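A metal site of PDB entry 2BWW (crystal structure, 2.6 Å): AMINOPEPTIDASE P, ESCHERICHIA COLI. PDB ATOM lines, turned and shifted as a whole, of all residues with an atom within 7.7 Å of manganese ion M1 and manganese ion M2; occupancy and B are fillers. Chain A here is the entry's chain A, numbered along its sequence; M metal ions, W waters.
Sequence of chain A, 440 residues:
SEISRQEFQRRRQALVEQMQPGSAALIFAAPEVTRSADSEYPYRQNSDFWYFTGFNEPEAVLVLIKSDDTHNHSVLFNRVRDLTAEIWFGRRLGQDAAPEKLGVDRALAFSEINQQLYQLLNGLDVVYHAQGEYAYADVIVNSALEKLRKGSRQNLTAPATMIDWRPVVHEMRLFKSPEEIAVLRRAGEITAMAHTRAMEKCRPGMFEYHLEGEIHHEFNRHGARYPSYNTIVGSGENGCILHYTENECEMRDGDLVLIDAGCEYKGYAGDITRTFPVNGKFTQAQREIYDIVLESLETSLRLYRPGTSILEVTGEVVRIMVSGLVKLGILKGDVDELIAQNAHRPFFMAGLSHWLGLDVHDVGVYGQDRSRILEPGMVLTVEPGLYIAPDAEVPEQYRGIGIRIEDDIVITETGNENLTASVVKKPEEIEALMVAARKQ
O of Thr 273 is in hydrogen-bond range of N of Glu 406 (2.9 Å). OH of Tyr 229 sits close to OD1 of Asp 271 (2.8 Å). The side-chain carboxylate (OD1) of Asp 260 sits close to the side-chain hydroxyl (OH) of Tyr 229 (2.6 Å). OD2 of Asp 260 lies close to NH2 of Arg 404 (3.0 Å). The side-chain carboxylate (OE2) of Glu 383 sits close to the side-chain hydroxyl (OG1) of Thr 381. The side-chain hydroxyl of Thr 273 sits at hydrogen-bond distance from the guanidinium group of Arg 404. OH of Tyr 229 lies within hydrogen-bond range of N of Gly 262. The backbone carbonyl oxygen (O) of Thr 381 lies within hydrogen-bond range of the side-chain hydroxyl (OG) of Ser 353 (2.6 Å).
Merely in contact with manganese ion M1: Tyr 229 (3.8 Å) and Thr 273 (3.6 Å). Five residues have an atom within 4 Å of manganese ion M1: Tyr 229, Asp 260, Asp 271, Thr 273 and Glu 406. The nearest printed residue that does not touch manganese ion M1 is Glu 383 (4.3 Å).
Residues that only touch manganese ion M2: Thr 381.
Manganese ion M1 is bound by the side-chain carboxylate (OD1) of Asp 271 (2.1 Å), the side-chain carboxylate (OE1) of Glu 406 (2.2 Å), the side-chain carboxylate (OD2) of Asp 260 (2.3 Å), water W1 (2.3 Å), the side-chain carboxylate (OD1) of Asp 260 (2.4 Å) and water W3 (2.4 Å).
Manganese ion M2 is bound by water W3 (2.0 Å), the side-chain carboxylate of Glu 406 (2.1 Å), a ring nitrogen (NE2) of His 354 (2.1 Å), the side-chain carboxylate of Asp 271 (2.2 Å) and the side-chain carboxylate of Glu 383 (2.4 Å). Manganese ion M2 has five donor atoms within binding distance.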
ATOM      1  N   TYR A 229     -19.879  22.771 -28.744  1.00  0.00           N
ATOM      2  CA  TYR A 229     -19.417  21.390 -28.593  1.00  0.00           C
ATOM      3  C   TYR A 229     -20.625  20.511 -28.259  1.00  0.00           C
ATOM      4  O   TYR A 229     -21.678  21.011 -27.882  1.00  0.00           O
ATOM      5  CB  TYR A 229     -18.332  21.264 -27.490  1.00  0.00           C
ATOM      6  CG  TYR A 229     -18.767  21.818 -26.158  1.00  0.00           C
ATOM      7  CD1 TYR A 229     -18.541  23.146 -25.828  1.00  0.00           C
ATOM      8  CD2 TYR A 229     -19.448  21.028 -25.238  1.00  0.00           C
ATOM      9  CE1 TYR A 229     -18.963  23.661 -24.635  1.00  0.00           C
ATOM     10  CE2 TYR A 229     -19.853  21.536 -24.018  1.00  0.00           C
ATOM     11  CZ  TYR A 229     -19.618  22.857 -23.724  1.00  0.00           C
ATOM     12  OH  TYR A 229     -20.025  23.392 -22.521  1.00  0.00           O
ATOM     13  N   ILE A 232     -23.286  17.426 -23.032  1.00  0.00           N
ATOM     14  CA  ILE A 232     -23.216  16.326 -22.083  1.00  0.00           C
ATOM     15  C   ILE A 232     -24.324  16.437 -21.043  1.00  0.00           C
ATOM     16  O   ILE A 232     -24.442  17.459 -20.369  1.00  0.00           O
ATOM     17  CB  ILE A 232     -21.868  16.351 -21.301  1.00  0.00           C
ATOM     18  CG1 ILE A 232     -20.665  16.105 -22.231  1.00  0.00           C
ATOM     19  CG2 ILE A 232     -21.888  15.331 -20.138  1.00  0.00           C
ATOM     20  CD1 ILE A 232     -19.315  16.470 -21.589  1.00  0.00           C
ATOM     21  N   LEU A 258     -25.062  15.877 -14.343  1.00  0.00           N
ATOM     22  CA  LEU A 258     -23.963  16.773 -14.726  1.00  0.00           C
ATOM     23  C   LEU A 258     -24.238  17.261 -16.150  1.00  0.00           C
ATOM     24  O   LEU A 258     -24.282  16.470 -17.098  1.00  0.00           O
ATOM     25  CB  LEU A 258     -22.650  16.009 -14.684  1.00  0.00           C
ATOM     26  CG  LEU A 258     -21.338  16.706 -15.025  1.00  0.00           C
ATOM     27  CD1 LEU A 258     -20.184  15.864 -14.518  1.00  0.00           C
ATOM     28  CD2 LEU A 258     -21.173  16.966 -16.521  1.00  0.00           C
ATOM     29  N   ILE A 259     -24.426  18.568 -16.284  1.00  0.00           N
ATOM     30  CA  ILE A 259     -24.711  19.171 -17.580  1.00  0.00           C
ATOM     31  C   ILE A 259     -23.574  20.070 -17.988  1.00  0.00           C
ATOM     32  O   ILE A 259     -23.293  21.076 -17.317  1.00  0.00           O
ATOM     33  CB  ILE A 259     -26.000  19.980 -17.573  1.00  0.00           C
ATOM     34  CG1 ILE A 259     -27.153  19.076 -17.148  1.00  0.00           C
ATOM     35  CG2 ILE A 259     -26.254  20.547 -18.960  1.00  0.00           C
ATOM     36  CD1 ILE A 259     -28.505  19.668 -17.341  1.00  0.00           C
ATOM     37  N   ASP A 260     -22.909  19.698 -19.082  1.00  0.00           N
ATOM     38  CA  ASP A 260     -21.883  20.523 -19.683  1.00  0.00           C
ATOM     39  C   ASP A 260     -22.346  20.886 -21.085  1.00  0.00           C
ATOM     40  O   ASP A 260     -22.377  20.044 -21.984  1.00  0.00           O
ATOM     41  CB  ASP A 260     -20.550  19.766 -19.709  1.00  0.00           C
ATOM     42  CG  ASP A 260     -19.358  20.644 -20.077  1.00  0.00           C
ATOM     43  OD1 ASP A 260     -19.515  21.797 -20.494  1.00  0.00           O
ATOM     44  OD2 ASP A 260     -18.231  20.145 -19.960  1.00  0.00           O
ATOM     45  N   ALA A 261     -22.739  22.155 -21.242  1.00  0.00           N
ATOM     46  CA  ALA A 261     -23.189  22.696 -22.505  1.00  0.00           C
ATOM     47  C   ALA A 261     -22.715  24.126 -22.710  1.00  0.00           C
ATOM     48  O   ALA A 261     -22.562  24.891 -21.734  1.00  0.00           O
ATOM     49  CB  ALA A 261     -24.697  22.631 -22.598  1.00  0.00           C
ATOM     50  N   GLY A 262     -22.481  24.473 -23.974  1.00  0.00           N
ATOM     51  CA  GLY A 262     -21.991  25.807 -24.361  1.00  0.00           C
ATOM     52  C   GLY A 262     -22.557  26.215 -25.701  1.00  0.00           C
ATOM     53  O   GLY A 262     -22.747  25.378 -26.584  1.00  0.00           O
ATOM     54  N   GLY A 270     -19.166  29.582 -25.467  1.00  0.00           N
ATOM     55  CA  GLY A 270     -19.451  29.481 -24.052  1.00  0.00           C
ATOM     56  C   GLY A 270     -19.135  28.054 -23.628  1.00  0.00           C
ATOM     57  O   GLY A 270     -19.097  27.139 -24.452  1.00  0.00           O
ATOM     58  N   ASP A 271     -18.888  27.875 -22.330  1.00  0.00           N
ATOM     59  CA  ASP A 271     -18.579  26.545 -21.804  1.00  0.00           C
ATOM     60  C   ASP A 271     -18.850  26.504 -20.299  1.00  0.00           C
ATOM     61  O   ASP A 271     -18.035  26.906 -19.506  1.00  0.00           O
ATOM     62  CB  ASP A 271     -17.115  26.183 -22.114  1.00  0.00           C
ATOM     63  CG  ASP A 271     -16.734  24.807 -21.639  1.00  0.00           C
ATOM     64  OD1 ASP A 271     -17.629  24.076 -21.164  1.00  0.00           O
ATOM     65  OD2 ASP A 271     -15.534  24.471 -21.731  1.00  0.00           O
ATOM     66  N   ILE A 272     -20.041  26.026 -19.936  1.00  0.00           N
ATOM     67  CA  ILE A 272     -20.465  25.949 -18.540  1.00  0.00           C
ATOM     68  C   ILE A 272     -20.785  24.505 -18.198  1.00  0.00           C
ATOM     69  O   ILE A 272     -21.324  23.746 -19.027  1.00  0.00           O
ATOM     70  CB  ILE A 272     -21.726  26.805 -18.312  1.00  0.00           C
ATOM     71  CG1 ILE A 272     -21.432  28.282 -18.541  1.00  0.00           C
ATOM     72  CG2 ILE A 272     -22.295  26.595 -16.904  1.00  0.00           C
ATOM     73  CD1 ILE A 272     -22.648  29.160 -18.394  1.00  0.00           C
ATOM     74  N   THR A 273     -20.458  24.122 -16.966  1.00  0.00           N
ATOM     75  CA  THR A 273     -20.927  22.844 -16.388  1.00  0.00           C
ATOM     76  C   THR A 273     -21.585  23.137 -15.068  1.00  0.00           C
ATOM     77  O   THR A 273     -21.027  23.863 -14.258  1.00  0.00           O
ATOM     78  CB  THR A 273     -19.821  21.819 -16.116  1.00  0.00           C
ATOM     79  OG1 THR A 273     -18.946  21.689 -17.258  1.00  0.00           O
ATOM     80  CG2 THR A 273     -20.441  20.461 -15.798  1.00  0.00           C
ATOM     81  N   GLY A 351      -7.762  18.361 -16.234  1.00  0.00           N
ATOM     82  CA  GLY A 351      -7.109  19.600 -15.828  1.00  0.00           C
ATOM     83  C   GLY A 351      -8.139  20.579 -15.276  1.00  0.00           C
ATOM     84  O   GLY A 351      -9.338  20.351 -15.392  1.00  0.00           O
ATOM     85  N   LEU A 352      -7.676  21.671 -14.694  1.00  0.00           N
ATOM     86  CA  LEU A 352      -8.544  22.697 -14.093  1.00  0.00           C
ATOM     87  C   LEU A 352      -9.071  23.734 -15.101  1.00  0.00           C
ATOM     88  O   LEU A 352     -10.131  24.335 -14.895  1.00  0.00           O
ATOM     89  CB  LEU A 352      -7.771  23.425 -12.990  1.00  0.00           C
ATOM     90  CG  LEU A 352      -8.515  24.514 -12.210  1.00  0.00           C
ATOM     91  CD1 LEU A 352      -9.628  23.933 -11.353  1.00  0.00           C
ATOM     92  CD2 LEU A 352      -7.557  25.334 -11.362  1.00  0.00           C
ATOM     93  N   SER A 353      -8.311  23.971 -16.175  1.00  0.00           N
ATOM     94  CA  SER A 353      -8.526  25.126 -17.038  1.00  0.00           C
ATOM     95  C   SER A 353      -8.013  24.900 -18.459  1.00  0.00           C
ATOM     96  O   SER A 353      -6.988  24.269 -18.686  1.00  0.00           O
ATOM     97  CB  SER A 353      -7.804  26.361 -16.467  1.00  0.00           C
ATOM     98  OG  SER A 353      -8.361  26.766 -15.209  1.00  0.00           O
ATOM     99  N   HIS A 354      -8.757  25.433 -19.425  1.00  0.00           N
ATOM    100  CA  HIS A 354      -8.246  25.561 -20.766  1.00  0.00           C
ATOM    101  C   HIS A 354      -8.583  26.922 -21.337  1.00  0.00           C
ATOM    102  O   HIS A 354      -9.540  27.546 -20.894  1.00  0.00           O
ATOM    103  CB  HIS A 354      -8.784  24.455 -21.669  1.00  0.00           C
ATOM    104  CG  HIS A 354     -10.273  24.387 -21.720  1.00  0.00           C
ATOM    105  ND1 HIS A 354     -11.049  25.282 -22.431  1.00  0.00           N
ATOM    106  CD2 HIS A 354     -11.135  23.485 -21.190  1.00  0.00           C
ATOM    107  CE1 HIS A 354     -12.327  24.953 -22.303  1.00  0.00           C
ATOM    108  NE2 HIS A 354     -12.408  23.861 -21.562  1.00  0.00           N
ATOM    109  N   TRP A 355      -7.794  27.376 -22.300  1.00  0.00           N
ATOM    110  CA  TRP A 355      -8.103  28.588 -23.018  1.00  0.00           C
ATOM    111  C   TRP A 355      -9.494  28.472 -23.654  1.00  0.00           C
ATOM    112  O   TRP A 355      -9.933  27.392 -24.054  1.00  0.00           O
ATOM    113  CB  TRP A 355      -7.071  28.858 -24.124  1.00  0.00           C
ATOM    114  CG  TRP A 355      -5.606  28.880 -23.705  1.00  0.00           C
ATOM    115  CD1 TRP A 355      -4.588  28.223 -24.315  1.00  0.00           C
ATOM    116  CD2 TRP A 355      -5.032  29.588 -22.615  1.00  0.00           C
ATOM    117  NE1 TRP A 355      -3.414  28.473 -23.675  1.00  0.00           N
ATOM    118  CE2 TRP A 355      -3.656  29.309 -22.618  1.00  0.00           C
ATOM    119  CE3 TRP A 355      -5.558  30.415 -21.620  1.00  0.00           C
ATOM    120  CZ2 TRP A 355      -2.777  29.849 -21.658  1.00  0.00           C
ATOM    121  CZ3 TRP A 355      -4.680  30.952 -20.673  1.00  0.00           C
ATOM    122  CH2 TRP A 355      -3.308  30.669 -20.705  1.00  0.00           C
ATOM    123  N   LEU A 356     -10.183  29.604 -23.754  1.00  0.00           N
ATOM    124  CA  LEU A 356     -11.500  29.651 -24.377  1.00  0.00           C
ATOM    125  C   LEU A 356     -11.529  30.779 -25.414  1.00  0.00           C
ATOM    126  O   LEU A 356     -10.960  31.833 -25.203  1.00  0.00           O
ATOM    127  CB  LEU A 356     -12.562  29.886 -23.317  1.00  0.00           C
ATOM    128  CG  LEU A 356     -14.028  29.783 -23.717  1.00  0.00           C
ATOM    129  CD1 LEU A 356     -14.394  28.357 -24.062  1.00  0.00           C
ATOM    130  CD2 LEU A 356     -14.904  30.317 -22.588  1.00  0.00           C
ATOM    131  N   VAL A 360     -13.713  26.090 -28.267  1.00  0.00           N
ATOM    132  CA  VAL A 360     -13.944  25.836 -26.844  1.00  0.00           C
ATOM    133  C   VAL A 360     -12.632  25.454 -26.152  1.00  0.00           C
ATOM    134  O   VAL A 360     -12.295  25.998 -25.100  1.00  0.00           O
ATOM    135  CB  VAL A 360     -15.079  24.801 -26.590  1.00  0.00           C
ATOM    136  CG1 VAL A 360     -14.751  23.456 -27.169  1.00  0.00           C
ATOM    137  CG2 VAL A 360     -15.363  24.671 -25.092  1.00  0.00           C
ATOM    138  N   HIS A 361     -11.869  24.549 -26.751  1.00  0.00           N
ATOM    139  CA  HIS A 361     -10.503  24.273 -26.317  1.00  0.00           C
ATOM    140  C   HIS A 361      -9.582  25.122 -27.133  1.00  0.00           C
ATOM    141  O   HIS A 361      -9.057  24.661 -28.157  1.00  0.00           O
ATOM    142  CB  HIS A 361     -10.157  22.802 -26.500  1.00  0.00           C
ATOM    143  CG  HIS A 361     -10.930  21.901 -25.598  1.00  0.00           C
ATOM    144  ND1 HIS A 361     -11.008  20.542 -25.788  1.00  0.00           N
ATOM    145  CD2 HIS A 361     -11.689  22.173 -24.502  1.00  0.00           C
ATOM    146  CE1 HIS A 361     -11.759  20.010 -24.832  1.00  0.00           C
ATOM    147  NE2 HIS A 361     -12.185  20.979 -24.048  1.00  0.00           N
ATOM    148  N   LEU A 380     -10.283  31.904 -20.073  1.00  0.00           N
ATOM    149  CA  LEU A 380     -10.123  30.517 -19.674  1.00  0.00           C
ATOM    150  C   LEU A 380     -11.272  29.984 -18.806  1.00  0.00           C
ATOM    151  O   LEU A 380     -12.045  30.756 -18.224  1.00  0.00           O
ATOM    152  CB  LEU A 380      -8.780  30.307 -18.959  1.00  0.00           C
ATOM    153  CG  LEU A 380      -8.535  31.098 -17.674  1.00  0.00           C
ATOM    154  CD1 LEU A 380      -7.500  30.386 -16.814  1.00  0.00           C
ATOM    155  CD2 LEU A 380      -8.109  32.532 -17.975  1.00  0.00           C
ATOM    156  N   THR A 381     -11.349  28.665 -18.759  1.00  0.00           N
ATOM    157  CA  THR A 381     -12.335  27.974 -17.943  1.00  0.00           C
ATOM    158  C   THR A 381     -11.750  27.612 -16.590  1.00  0.00           C
ATOM    159  O   THR A 381     -10.533  27.488 -16.440  1.00  0.00           O
ATOM    160  CB  THR A 381     -12.826  26.704 -18.620  1.00  0.00           C
ATOM    161  OG1 THR A 381     -11.740  25.761 -18.723  1.00  0.00           O
ATOM    162  CG2 THR A 381     -13.361  27.036 -20.002  1.00  0.00           C
ATOM    163  N   VAL A 382     -12.627  27.490 -15.606  1.00  0.00           N
ATOM    164  CA  VAL A 382     -12.268  26.990 -14.289  1.00  0.00           C
ATOM    165  C   VAL A 382     -13.240  25.856 -14.030  1.00  0.00           C
ATOM    166  O   VAL A 382     -14.443  26.097 -13.889  1.00  0.00           O
ATOM    167  CB  VAL A 382     -12.379  28.080 -13.202  1.00  0.00           C
ATOM    168  CG1 VAL A 382     -11.667  27.619 -11.934  1.00  0.00           C
ATOM    169  CG2 VAL A 382     -11.775  29.407 -13.693  1.00  0.00           C
ATOM    170  N   GLU A 383     -12.741  24.628 -13.991  1.00  0.00           N
ATOM    171  CA  GLU A 383     -13.645  23.481 -14.017  1.00  0.00           C
ATOM    172  C   GLU A 383     -13.175  22.285 -13.182  1.00  0.00           C
ATOM    173  O   GLU A 383     -12.929  21.202 -13.717  1.00  0.00           O
ATOM    174  CB  GLU A 383     -13.899  23.074 -15.484  1.00  0.00           C
ATOM    175  CG  GLU A 383     -12.647  22.787 -16.321  1.00  0.00           C
ATOM    176  CD  GLU A 383     -12.982  22.415 -17.756  1.00  0.00           C
ATOM    177  OE1 GLU A 383     -13.676  21.385 -17.964  1.00  0.00           O
ATOM    178  OE2 GLU A 383     -12.568  23.171 -18.672  1.00  0.00           O
ATOM    179  N   ARG A 404     -19.007  18.072 -11.632  1.00  0.00           N
ATOM    180  CA  ARG A 404     -18.150  19.156 -12.130  1.00  0.00           C
ATOM    181  C   ARG A 404     -18.906  20.460 -12.075  1.00  0.00           C
ATOM    182  O   ARG A 404     -20.110  20.495 -12.335  1.00  0.00           O
ATOM    183  CB  ARG A 404     -17.703  18.876 -13.551  1.00  0.00           C
ATOM    184  CG  ARG A 404     -16.878  19.996 -14.180  1.00  0.00           C
ATOM    185  CD  ARG A 404     -16.144  19.533 -15.448  1.00  0.00           C
ATOM    186  NE  ARG A 404     -17.038  19.221 -16.560  1.00  0.00           N
ATOM    187  CZ  ARG A 404     -17.292  18.004 -17.032  1.00  0.00           C
ATOM    188  NH1 ARG A 404     -16.762  16.914 -16.483  1.00  0.00           N
ATOM    189  NH2 ARG A 404     -18.103  17.857 -18.068  1.00  0.00           N
ATOM    190  N   GLU A 406     -18.223  24.299 -13.720  1.00  0.00           N
ATOM    191  CA  GLU A 406     -17.346  25.008 -14.649  1.00  0.00           C
ATOM    192  C   GLU A 406     -17.877  26.411 -14.925  1.00  0.00           C
ATOM    193  O   GLU A 406     -19.057  26.580 -15.214  1.00  0.00           O
ATOM    194  CB  GLU A 406     -17.206  24.208 -15.952  1.00  0.00           C
ATOM    195  CG  GLU A 406     -16.601  24.975 -17.133  1.00  0.00           C
ATOM    196  CD  GLU A 406     -16.222  24.071 -18.295  1.00  0.00           C
ATOM    197  OE1 GLU A 406     -16.896  23.028 -18.468  1.00  0.00           O
ATOM    198  OE2 GLU A 406     -15.267  24.410 -19.045  1.00  0.00           O
ATOM    199  N   ASP A 407     -16.987  27.399 -14.789  1.00  0.00           N
ATOM    200  CA  ASP A 407     -17.244  28.791 -15.107  1.00  0.00           C
ATOM    201  C   ASP A 407     -16.196  29.281 -16.109  1.00  0.00           C
ATOM    202  O   ASP A 407     -15.104  28.694 -16.213  1.00  0.00           O
ATOM    203  CB  ASP A 407     -17.157  29.660 -13.844  1.00  0.00           C
ATOM    204  CG  ASP A 407     -18.509  29.837 -13.140  1.00  0.00           C
ATOM    205  OD1 ASP A 407     -19.558  29.655 -13.781  1.00  0.00           O
ATOM    206  OD2 ASP A 407     -18.515  30.199 -11.941  1.00  0.00           O
ATOM    207  N   ASP A 408     -16.523  30.358 -16.828  1.00  0.00           N
ATOM    208  CA  ASP A 408     -15.626  30.984 -17.812  1.00  0.00           C
ATOM    209  C   ASP A 408     -15.204  32.357 -17.293  1.00  0.00           C
ATOM    210  O   ASP A 408     -16.050  33.157 -16.843  1.00  0.00           O
ATOM    211  CB  ASP A 408     -16.322  31.141 -19.168  1.00  0.00           C
ATOM    212  CG  ASP A 408     -16.904  29.822 -19.713  1.00  0.00           C
ATOM    213  OD1 ASP A 408     -16.420  28.719 -19.352  1.00  0.00           O
ATOM    214  OD2 ASP A 408     -17.870  29.895 -20.499  1.00  0.00           O
HETATM  215 MN    MN M   1     -17.178  22.110 -20.421  1.00  0.00          MN
HETATM  216 MN    MN M   2     -14.185  23.361 -20.468  1.00  0.00          MN
HETATM  217  O   HOH W   1     -16.786  21.360 -22.561  1.00  0.00           O
HETATM  218  O   HOH W   2     -14.310  21.203 -22.631  1.00  0.00           O
HETATM  219  O   HOH W   3     -14.873  21.502 -20.246  1.00  0.00           O
